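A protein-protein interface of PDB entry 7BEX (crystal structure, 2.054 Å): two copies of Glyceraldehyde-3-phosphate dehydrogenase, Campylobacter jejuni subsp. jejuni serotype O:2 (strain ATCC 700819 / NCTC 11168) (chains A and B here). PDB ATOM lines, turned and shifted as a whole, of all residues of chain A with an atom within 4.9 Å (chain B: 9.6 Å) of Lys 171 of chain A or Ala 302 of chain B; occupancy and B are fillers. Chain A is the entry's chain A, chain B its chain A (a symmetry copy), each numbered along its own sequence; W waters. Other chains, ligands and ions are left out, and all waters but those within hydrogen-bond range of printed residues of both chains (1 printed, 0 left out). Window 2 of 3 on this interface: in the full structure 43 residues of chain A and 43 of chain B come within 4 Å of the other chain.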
ATOM      1  N   ILE A 169     -20.350  16.470  -0.646  1.00  0.00           N
ATOM      2  CA  ILE A 169     -20.743  17.801  -1.185  1.00  0.00           C
ATOM      3  C   ILE A 169     -20.870  18.790  -0.047  1.00  0.00           C
ATOM      4  O   ILE A 169     -21.643  18.534   0.839  1.00  0.00           O
ATOM      5  CB  ILE A 169     -22.054  17.742  -1.983  1.00  0.00           C
ATOM      6  CG1 ILE A 169     -21.985  16.784  -3.178  1.00  0.00           C
ATOM      7  CG2 ILE A 169     -22.443  19.140  -2.383  1.00  0.00           C
ATOM      8  CD1 ILE A 169     -23.317  16.493  -3.841  1.00  0.00           C
ATOM      9  N   GLU A 170     -20.078  19.856  -0.086  1.00  0.00           N
ATOM     10  CA  GLU A 170     -20.105  20.918   0.944  1.00  0.00           C
ATOM     11  C   GLU A 170     -21.178  21.918   0.519  1.00  0.00           C
ATOM     12  O   GLU A 170     -21.974  22.363   1.385  1.00  0.00           O
ATOM     13  CB  GLU A 170     -18.719  21.569   1.063  1.00  0.00           C
ATOM     14  CG  GLU A 170     -17.664  20.623   1.612  1.00  0.00           C
ATOM     15  CD  GLU A 170     -17.928  20.159   3.035  1.00  0.00           C
ATOM     16  OE1 GLU A 170     -18.403  20.950   3.787  1.00  0.00           O
ATOM     17  OE2 GLU A 170     -17.704  19.000   3.357  1.00  0.00           O
ATOM     18  N   LYS A 171     -21.168  22.303  -0.762  1.00  0.00           N
ATOM     19  CA  LYS A 171     -22.137  23.291  -1.271  1.00  0.00           C
ATOM     20  C   LYS A 171     -22.086  23.318  -2.793  1.00  0.00           C
ATOM     21  O   LYS A 171     -21.066  22.876  -3.351  1.00  0.00           O
ATOM     22  CB  LYS A 171     -21.796  24.655  -0.683  1.00  0.00           C
ATOM     23  CG  LYS A 171     -20.332  25.019  -0.806  1.00  0.00           C
ATOM     24  CD  LYS A 171     -19.941  26.263  -0.072  1.00  0.00           C
ATOM     25  CE  LYS A 171     -19.329  25.962   1.270  1.00  0.00           C
ATOM     26  NZ  LYS A 171     -19.028  27.213   1.977  1.00  0.00           N
ATOM     27  N   GLY A 172     -23.142  23.823  -3.434  1.00  0.00           N
ATOM     28  CA  GLY A 172     -23.143  23.898  -4.903  1.00  0.00           C
ATOM     29  C   GLY A 172     -24.301  24.709  -5.435  1.00  0.00           C
ATOM     30  O   GLY A 172     -25.282  24.955  -4.673  1.00  0.00           O
ATOM     31  N   LEU A 173     -24.149  25.160  -6.680  1.00  0.00           N
ATOM     32  CA  LEU A 173     -25.175  25.938  -7.393  1.00  0.00           C
ATOM     33  C   LEU A 173     -25.287  25.345  -8.796  1.00  0.00           C
ATOM     34  O   LEU A 173     -24.255  24.903  -9.363  1.00  0.00           O
ATOM     35  CB  LEU A 173     -24.775  27.413  -7.372  1.00  0.00           C
ATOM     36  CG  LEU A 173     -24.836  28.116  -6.010  1.00  0.00           C
ATOM     37  CD1 LEU A 173     -24.252  29.519  -6.108  1.00  0.00           C
ATOM     38  CD2 LEU A 173     -26.271  28.176  -5.554  1.00  0.00           C
ATOM     39  N   LYS A 225     -27.633  23.094   1.240  1.00  0.00           N
ATOM     40  CA  LYS A 225     -26.315  23.165   0.553  1.00  0.00           C
ATOM     41  C   LYS A 225     -26.409  23.437  -0.954  1.00  0.00           C
ATOM     42  O   LYS A 225     -25.349  23.553  -1.565  1.00  0.00           O
ATOM     43  CB  LYS A 225     -25.581  21.860   0.799  1.00  0.00           C
ATOM     44  CG  LYS A 225     -25.174  21.736   2.256  1.00  0.00           C
ATOM     45  CD  LYS A 225     -24.594  20.405   2.535  1.00  0.00           C
ATOM     46  CE  LYS A 225     -24.096  20.285   3.958  1.00  0.00           C
ATOM     47  NZ  LYS A 225     -23.355  19.015   4.048  1.00  0.00           N
ATOM     48  N   LEU A 226     -27.591  23.467  -1.554  1.00  0.00           N
ATOM     49  CA  LEU A 226     -27.744  23.600  -3.037  1.00  0.00           C
ATOM     50  C   LEU A 226     -28.833  24.624  -3.321  1.00  0.00           C
ATOM     51  O   LEU A 226     -29.839  24.654  -2.572  1.00  0.00           O
ATOM     52  CB  LEU A 226     -28.185  22.292  -3.693  1.00  0.00           C
ATOM     53  CG  LEU A 226     -27.242  21.103  -3.684  1.00  0.00           C
ATOM     54  CD1 LEU A 226     -27.816  19.955  -4.498  1.00  0.00           C
ATOM     55  CD2 LEU A 226     -25.863  21.481  -4.214  1.00  0.00           C
ATOM     56  N   THR A 244     -22.083  23.174 -10.267  1.00  0.00           N
ATOM     57  CA  THR A 244     -20.780  23.637  -9.757  1.00  0.00           C
ATOM     58  C   THR A 244     -20.807  23.436  -8.265  1.00  0.00           C
ATOM     59  O   THR A 244     -21.757  23.870  -7.670  1.00  0.00           O
ATOM     60  CB  THR A 244     -20.454  25.088 -10.112  1.00  0.00           C
ATOM     61  OG1 THR A 244     -20.683  25.307 -11.495  1.00  0.00           O
ATOM     62  CG2 THR A 244     -19.013  25.403  -9.776  1.00  0.00           C
ATOM     63  N   ALA A 245     -19.845  22.707  -7.711  1.00  0.00           N
ATOM     64  CA  ALA A 245     -19.916  22.290  -6.304  1.00  0.00           C
ATOM     65  C   ALA A 245     -18.528  22.382  -5.668  1.00  0.00           C
ATOM     66  O   ALA A 245     -17.509  22.229  -6.353  1.00  0.00           O
ATOM     67  CB  ALA A 245     -20.517  20.909  -6.240  1.00  0.00           C
ATOM     68  N   GLN A 246     -18.502  22.637  -4.384  1.00  0.00           N
ATOM     69  CA  GLN A 246     -17.302  22.431  -3.548  1.00  0.00           C
ATOM     70  C   GLN A 246     -17.463  21.092  -2.837  1.00  0.00           C
ATOM     71  O   GLN A 246     -18.468  20.902  -2.126  1.00  0.00           O
ATOM     72  CB  GLN A 246     -17.147  23.573  -2.554  1.00  0.00           C
ATOM     73  CG  GLN A 246     -15.949  23.448  -1.630  1.00  0.00           C
ATOM     74  CD  GLN A 246     -16.095  24.460  -0.506  1.00  0.00           C
ATOM     75  OE1 GLN A 246     -16.487  25.609  -0.694  1.00  0.00           O
ATOM     76  NE2 GLN A 246     -15.699  24.071   0.678  1.00  0.00           N
ATOM     77  N   LYS B 171     -11.732  31.078  -5.932  1.00  0.00           N
ATOM     78  CA  LYS B 171     -11.758  30.175  -7.096  1.00  0.00           C
ATOM     79  C   LYS B 171     -13.119  30.258  -7.777  1.00  0.00           C
ATOM     80  O   LYS B 171     -14.077  30.694  -7.114  1.00  0.00           O
ATOM     81  CB  LYS B 171     -11.466  28.757  -6.618  1.00  0.00           C
ATOM     82  CG  LYS B 171     -12.290  28.339  -5.420  1.00  0.00           C
ATOM     83  CD  LYS B 171     -11.888  27.028  -4.820  1.00  0.00           C
ATOM     84  CE  LYS B 171     -10.992  27.202  -3.623  1.00  0.00           C
ATOM     85  NZ  LYS B 171     -10.571  25.891  -3.116  1.00  0.00           N
ATOM     86  N   THR B 244     -19.667  30.953 -11.314  1.00  0.00           N
ATOM     87  CA  THR B 244     -19.864  30.397  -9.963  1.00  0.00           C
ATOM     88  C   THR B 244     -18.534  30.488  -9.263  1.00  0.00           C
ATOM     89  O   THR B 244     -17.577  30.053  -9.846  1.00  0.00           O
ATOM     90  CB  THR B 244     -20.395  28.963  -9.953  1.00  0.00           C
ATOM     91  OG1 THR B 244     -21.507  28.856 -10.827  1.00  0.00           O
ATOM     92  CG2 THR B 244     -20.804  28.560  -8.554  1.00  0.00           C
ATOM     93  N   ALA B 245     -18.477  31.131  -8.102  1.00  0.00           N
ATOM     94  CA  ALA B 245     -17.190  31.445  -7.466  1.00  0.00           C
ATOM     95  C   ALA B 245     -17.302  31.247  -5.953  1.00  0.00           C
ATOM     96  O   ALA B 245     -18.383  31.405  -5.373  1.00  0.00           O
ATOM     97  CB  ALA B 245     -16.787  32.843  -7.861  1.00  0.00           C
ATOM     98  N   GLN B 246     -16.199  30.896  -5.340  1.00  0.00           N
ATOM     99  CA  GLN B 246     -16.032  30.987  -3.875  1.00  0.00           C
ATOM    100  C   GLN B 246     -15.273  32.275  -3.580  1.00  0.00           C
ATOM    101  O   GLN B 246     -14.160  32.456  -4.109  1.00  0.00           O
ATOM    102  CB  GLN B 246     -15.285  29.769  -3.351  1.00  0.00           C
ATOM    103  CG  GLN B 246     -15.043  29.773  -1.852  1.00  0.00           C
ATOM    104  CD  GLN B 246     -14.032  28.688  -1.520  1.00  0.00           C
ATOM    105  OE1 GLN B 246     -14.059  27.575  -2.039  1.00  0.00           O
ATOM    106  NE2 GLN B 246     -13.166  28.971  -0.583  1.00  0.00           N
ATOM    107  N   LEU B 247     -15.909  33.190  -2.850  1.00  0.00           N
ATOM    108  CA  LEU B 247     -15.305  34.480  -2.425  1.00  0.00           C
ATOM    109  C   LEU B 247     -14.537  34.293  -1.096  1.00  0.00           C
ATOM    110  O   LEU B 247     -14.749  33.277  -0.420  1.00  0.00           O
ATOM    111  CB  LEU B 247     -16.407  35.529  -2.287  1.00  0.00           C
ATOM    112  CG  LEU B 247     -17.272  35.726  -3.540  1.00  0.00           C
ATOM    113  CD1 LEU B 247     -18.204  36.926  -3.381  1.00  0.00           C
ATOM    114  CD2 LEU B 247     -16.426  35.905  -4.778  1.00  0.00           C
ATOM    115  N   ARG B 249     -14.837  35.909   1.686  1.00  0.00           N
ATOM    116  CA  ARG B 249     -15.636  36.167   2.913  1.00  0.00           C
ATOM    117  C   ARG B 249     -17.112  35.962   2.608  1.00  0.00           C
ATOM    118  O   ARG B 249     -17.458  35.843   1.412  1.00  0.00           O
ATOM    119  CB  ARG B 249     -15.352  37.580   3.438  1.00  0.00           C
ATOM    120  CG  ARG B 249     -15.728  38.677   2.452  1.00  0.00           C
ATOM    121  CD  ARG B 249     -16.042  39.919   3.238  1.00  0.00           C
ATOM    122  NE  ARG B 249     -16.412  41.142   2.537  1.00  0.00           N
ATOM    123  CZ  ARG B 249     -17.653  41.635   2.430  1.00  0.00           C
ATOM    124  NH1 ARG B 249     -18.717  40.955   2.803  1.00  0.00           N
ATOM    125  NH2 ARG B 249     -17.819  42.813   1.863  1.00  0.00           N
ATOM    126  N   LYS B 250     -17.923  35.906   3.668  1.00  0.00           N
ATOM    127  CA  LYS B 250     -19.394  35.820   3.585  1.00  0.00           C
ATOM    128  C   LYS B 250     -19.883  37.098   2.920  1.00  0.00           C
ATOM    129  O   LYS B 250     -19.369  38.183   3.253  1.00  0.00           O
ATOM    130  CB  LYS B 250     -20.028  35.610   4.961  1.00  0.00           C
ATOM    131  CG  LYS B 250     -21.553  35.619   5.004  1.00  0.00           C
ATOM    132  CD  LYS B 250     -22.051  35.180   6.370  1.00  0.00           C
ATOM    133  CE  LYS B 250     -23.564  35.109   6.545  1.00  0.00           C
ATOM    134  NZ  LYS B 250     -23.884  34.556   7.894  1.00  0.00           N
ATOM    135  N   VAL B 251     -20.808  36.934   1.980  1.00  0.00           N
ATOM    136  CA  VAL B 251     -21.512  38.047   1.314  1.00  0.00           C
ATOM    137  C   VAL B 251     -22.998  37.709   1.269  1.00  0.00           C
ATOM    138  O   VAL B 251     -23.354  36.501   1.438  1.00  0.00           O
ATOM    139  CB  VAL B 251     -20.933  38.275  -0.092  1.00  0.00           C
ATOM    140  CG1 VAL B 251     -19.460  38.592  -0.008  1.00  0.00           C
ATOM    141  CG2 VAL B 251     -21.195  37.084  -1.009  1.00  0.00           C
ATOM    142  N   SER B 252     -23.816  38.719   0.966  1.00  0.00           N
ATOM    143  CA  SER B 252     -25.244  38.533   0.637  1.00  0.00           C
ATOM    144  C   SER B 252     -25.481  38.811  -0.856  1.00  0.00           C
ATOM    145  O   SER B 252     -24.702  39.520  -1.513  1.00  0.00           O
ATOM    146  CB  SER B 252     -26.086  39.407   1.501  1.00  0.00           C
ATOM    147  OG  SER B 252     -25.944  40.761   1.091  1.00  0.00           O
ATOM    148  N   GLN B 299     -27.091  34.582  -6.930  1.00  0.00           N
ATOM    149  CA  GLN B 299     -27.345  33.606  -5.838  1.00  0.00           C
ATOM    150  C   GLN B 299     -26.118  33.486  -4.931  1.00  0.00           C
ATOM    151  O   GLN B 299     -24.976  33.625  -5.429  1.00  0.00           O
ATOM    152  CB  GLN B 299     -27.797  32.256  -6.400  1.00  0.00           C
ATOM    153  CG  GLN B 299     -29.170  32.290  -7.053  1.00  0.00           C
ATOM    154  CD  GLN B 299     -29.513  30.935  -7.650  1.00  0.00           C
ATOM    155  OE1 GLN B 299     -28.771  30.378  -8.444  1.00  0.00           O
ATOM    156  NE2 GLN B 299     -30.617  30.342  -7.236  1.00  0.00           N
ATOM    157  N   VAL B 300     -26.376  33.234  -3.642  1.00  0.00           N
ATOM    158  CA  VAL B 300     -25.351  32.903  -2.609  1.00  0.00           C
ATOM    159  C   VAL B 300     -25.842  31.680  -1.829  1.00  0.00           C
ATOM    160  O   VAL B 300     -27.006  31.672  -1.381  1.00  0.00           O
ATOM    161  CB  VAL B 300     -25.104  34.069  -1.641  1.00  0.00           C
ATOM    162  CG1 VAL B 300     -23.947  33.742  -0.690  1.00  0.00           C
ATOM    163  CG2 VAL B 300     -24.867  35.355  -2.387  1.00  0.00           C
ATOM    164  N   ILE B 301     -24.965  30.708  -1.599  1.00  0.00           N
ATOM    165  CA  ILE B 301     -25.292  29.603  -0.657  1.00  0.00           C
ATOM    166  C   ILE B 301     -24.120  29.450   0.301  1.00  0.00           C
ATOM    167  O   ILE B 301     -22.966  29.691  -0.111  1.00  0.00           O
ATOM    168  CB  ILE B 301     -25.668  28.322  -1.424  1.00  0.00           C
ATOM    169  CG1 ILE B 301     -26.168  27.207  -0.511  1.00  0.00           C
ATOM    170  CG2 ILE B 301     -24.543  27.805  -2.287  1.00  0.00           C
ATOM    171  CD1 ILE B 301     -27.613  27.237  -0.289  1.00  0.00           C
ATOM    172  N   ALA B 302     -24.409  29.089   1.558  1.00  0.00           N
ATOM    173  CA  ALA B 302     -23.363  28.689   2.532  1.00  0.00           C
ATOM    174  C   ALA B 302     -22.292  29.777   2.594  1.00  0.00           C
ATOM    175  O   ALA B 302     -21.121  29.454   2.488  1.00  0.00           O
ATOM    176  CB  ALA B 302     -22.788  27.370   2.092  1.00  0.00           C
ATOM    177  N   ASP B 303     -22.727  31.043   2.667  1.00  0.00           N
ATOM    178  CA  ASP B 303     -21.929  32.252   2.997  1.00  0.00           C
ATOM    179  C   ASP B 303     -21.138  32.782   1.799  1.00  0.00           C
ATOM    180  O   ASP B 303     -21.226  33.993   1.570  1.00  0.00           O
ATOM    181  CB  ASP B 303     -20.982  32.034   4.173  1.00  0.00           C
ATOM    182  CG  ASP B 303     -21.679  31.658   5.483  1.00  0.00           C
ATOM    183  OD1 ASP B 303     -22.899  31.856   5.628  1.00  0.00           O
ATOM    184  OD2 ASP B 303     -20.981  31.206   6.362  1.00  0.00           O
ATOM    185  N   ASP B 304     -20.308  31.957   1.156  1.00  0.00           N
ATOM    186  CA  ASP B 304     -19.214  32.461   0.295  1.00  0.00           C
ATOM    187  C   ASP B 304     -19.287  31.905  -1.130  1.00  0.00           C
ATOM    188  O   ASP B 304     -18.335  32.160  -1.896  1.00  0.00           O
ATOM    189  CB  ASP B 304     -17.881  32.107   0.949  1.00  0.00           C
ATOM    190  CG  ASP B 304     -17.521  30.626   0.985  1.00  0.00           C
ATOM    191  OD1 ASP B 304     -18.346  29.732   0.606  1.00  0.00           O
ATOM    192  OD2 ASP B 304     -16.412  30.365   1.437  1.00  0.00           O
ATOM    193  N   PHE B 305     -20.356  31.190  -1.473  1.00  0.00           N
ATOM    194  CA  PHE B 305     -20.445  30.411  -2.730  1.00  0.00           C
ATOM    195  C   PHE B 305     -21.535  31.062  -3.584  1.00  0.00           C
ATOM    196  O   PHE B 305     -22.727  31.064  -3.149  1.00  0.00           O
ATOM    197  CB  PHE B 305     -20.649  28.933  -2.405  1.00  0.00           C
ATOM    198  CG  PHE B 305     -20.431  27.989  -3.552  1.00  0.00           C
ATOM    199  CD1 PHE B 305     -21.388  27.863  -4.555  1.00  0.00           C
ATOM    200  CD2 PHE B 305     -19.255  27.253  -3.651  1.00  0.00           C
ATOM    201  CE1 PHE B 305     -21.181  26.983  -5.611  1.00  0.00           C
ATOM    202  CE2 PHE B 305     -19.046  26.361  -4.697  1.00  0.00           C
ATOM    203  CZ  PHE B 305     -20.005  26.242  -5.688  1.00  0.00           C
ATOM    204  N   ILE B 306     -21.137  31.681  -4.697  1.00  0.00           N
ATOM    205  CA  ILE B 306     -22.001  32.669  -5.401  1.00  0.00           C
ATOM    206  C   ILE B 306     -22.153  32.278  -6.865  1.00  0.00           C
ATOM    207  O   ILE B 306     -21.233  31.598  -7.436  1.00  0.00           O
ATOM    208  CB  ILE B 306     -21.433  34.098  -5.204  1.00  0.00           C
ATOM    209  CG1 ILE B 306     -20.149  34.343  -5.984  1.00  0.00           C
ATOM    210  CG2 ILE B 306     -21.158  34.342  -3.726  1.00  0.00           C
ATOM    211  CD1 ILE B 306     -20.314  35.022  -7.242  1.00  0.00           C
HETATM  212  O   HOH W   1     -16.722  27.401   1.095  1.00  0.00           O
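NZ of Lys 171 of chain A is in hydrogen-bond range of O of Ala 302 of chain B (3.1 Å).
The side-chain amino group (NZ) of Lys 171 of chain A lies within salt-bridge range of the side-chain carboxylate (OD1) of Asp 304 of chain B (2.9 Å).
The side-chain amide oxygen (OE1) of Gln 246 of chain A sits close to the side-chain amide oxygen (OE1) of Gln 246 of chain B (3.4 Å).
The backbone carbonyl oxygen (O) of Asp 304 of chain B is in hydrogen-bond range of the backbone NH (N) of Leu 247 of chain B.
The backbone NH of Gly 172 of chain A sits at hydrogen-bond distance from the backbone carbonyl oxygen of Lys 225 of chain A.
The backbone carbonyl oxygen of Lys 171 of chain A is in hydrogen-bond range of the backbone NH of Gln 246 of chain A (2.8 Å).
N of Glu 170 of chain A sits at hydrogen-bond distance from O of Gln 246 of chain A, at 2.8 Å.
The backbone NH of Leu 173 of chain A sits at hydrogen-bond distance from the backbone carbonyl oxygen of Thr 244 of chain A (2.9 Å).
The backbone NH (N) of Gln 246 of chain B lies within hydrogen-bond range of the backbone carbonyl oxygen (O) of Lys 171 of chain B.
Of the printed residues of chain B, Lys 171 of chain A touches Ala 302 (3.1 Å), Asp 304 (2.9 Å) and Phe 305 (3.6 Å).
Gly 172 of chain A touches just these residues of chain B: Ile 301 and Phe 305.
Printed residues of chain B within 4 Å of Lys 225 of chain A: Ile 301.
Of the printed residues of chain B, Thr 244 of chain A touches Thr 244 (3.7 Å) and Phe 305 (3.6 Å).
Of chain A, only Lys 171 comes within 4 Å of Ala 302 of chain B.
Among the printed residues, merely in contact across the chains: Leu 173 of chain A with Ile 306 of chain B (3.5 Å), Thr 244 of chain A with Phe 305 of chain B (3.6 Å), Lys 171 of chain A with Phe 305 of chain B (3.6 Å), Leu 173 of chain A with Phe 305 of chain B (3.6 Å), Thr 244 of chain A with Thr 244 of chain B (3.7 Å), Leu 173 of chain A with Ile 301 of chain B (3.7 Å), Gly 172 of chain A with Phe 305 of chain B (3.7 Å), Gln 246 of chain A with Phe 305 of chain B (3.8 Å), Gly 172 of chain A with Ile 301 of chain B (3.8 Å), Lys 225 of chain A with Ile 301 of chain B (3.8 Å) and Leu 226 of chain A with Ile 301 of chain B (3.98 Å).
Thr 244 of chain A touches its own counterpart, Thr 244 of chain B.
Gln 246 of chain A touches its own counterpart, Gln 246 of chain B.
Positions printed for both chains: 171, 244, 245 and 246.
Water W1 lies within hydrogen-bond range of NZ of Lys 171 of chain A, OE1 of Gln 246 of chain A and OD1 of Asp 304 of chain B.
Printed residues of chain B that touch a printed residue of chain A: Thr 244, Gln 246, Ile 301, Ala 302, Asp 304, Phe 305 and Ile 306.
Of the 10 printed residues of chain A, 7 touch a printed residue of chain B.
Hydrophobic or aromatic side chains of chain A that line the printed part of chain B: Leu 173.
Among the printed residues, 14 pairs touch across the chains.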
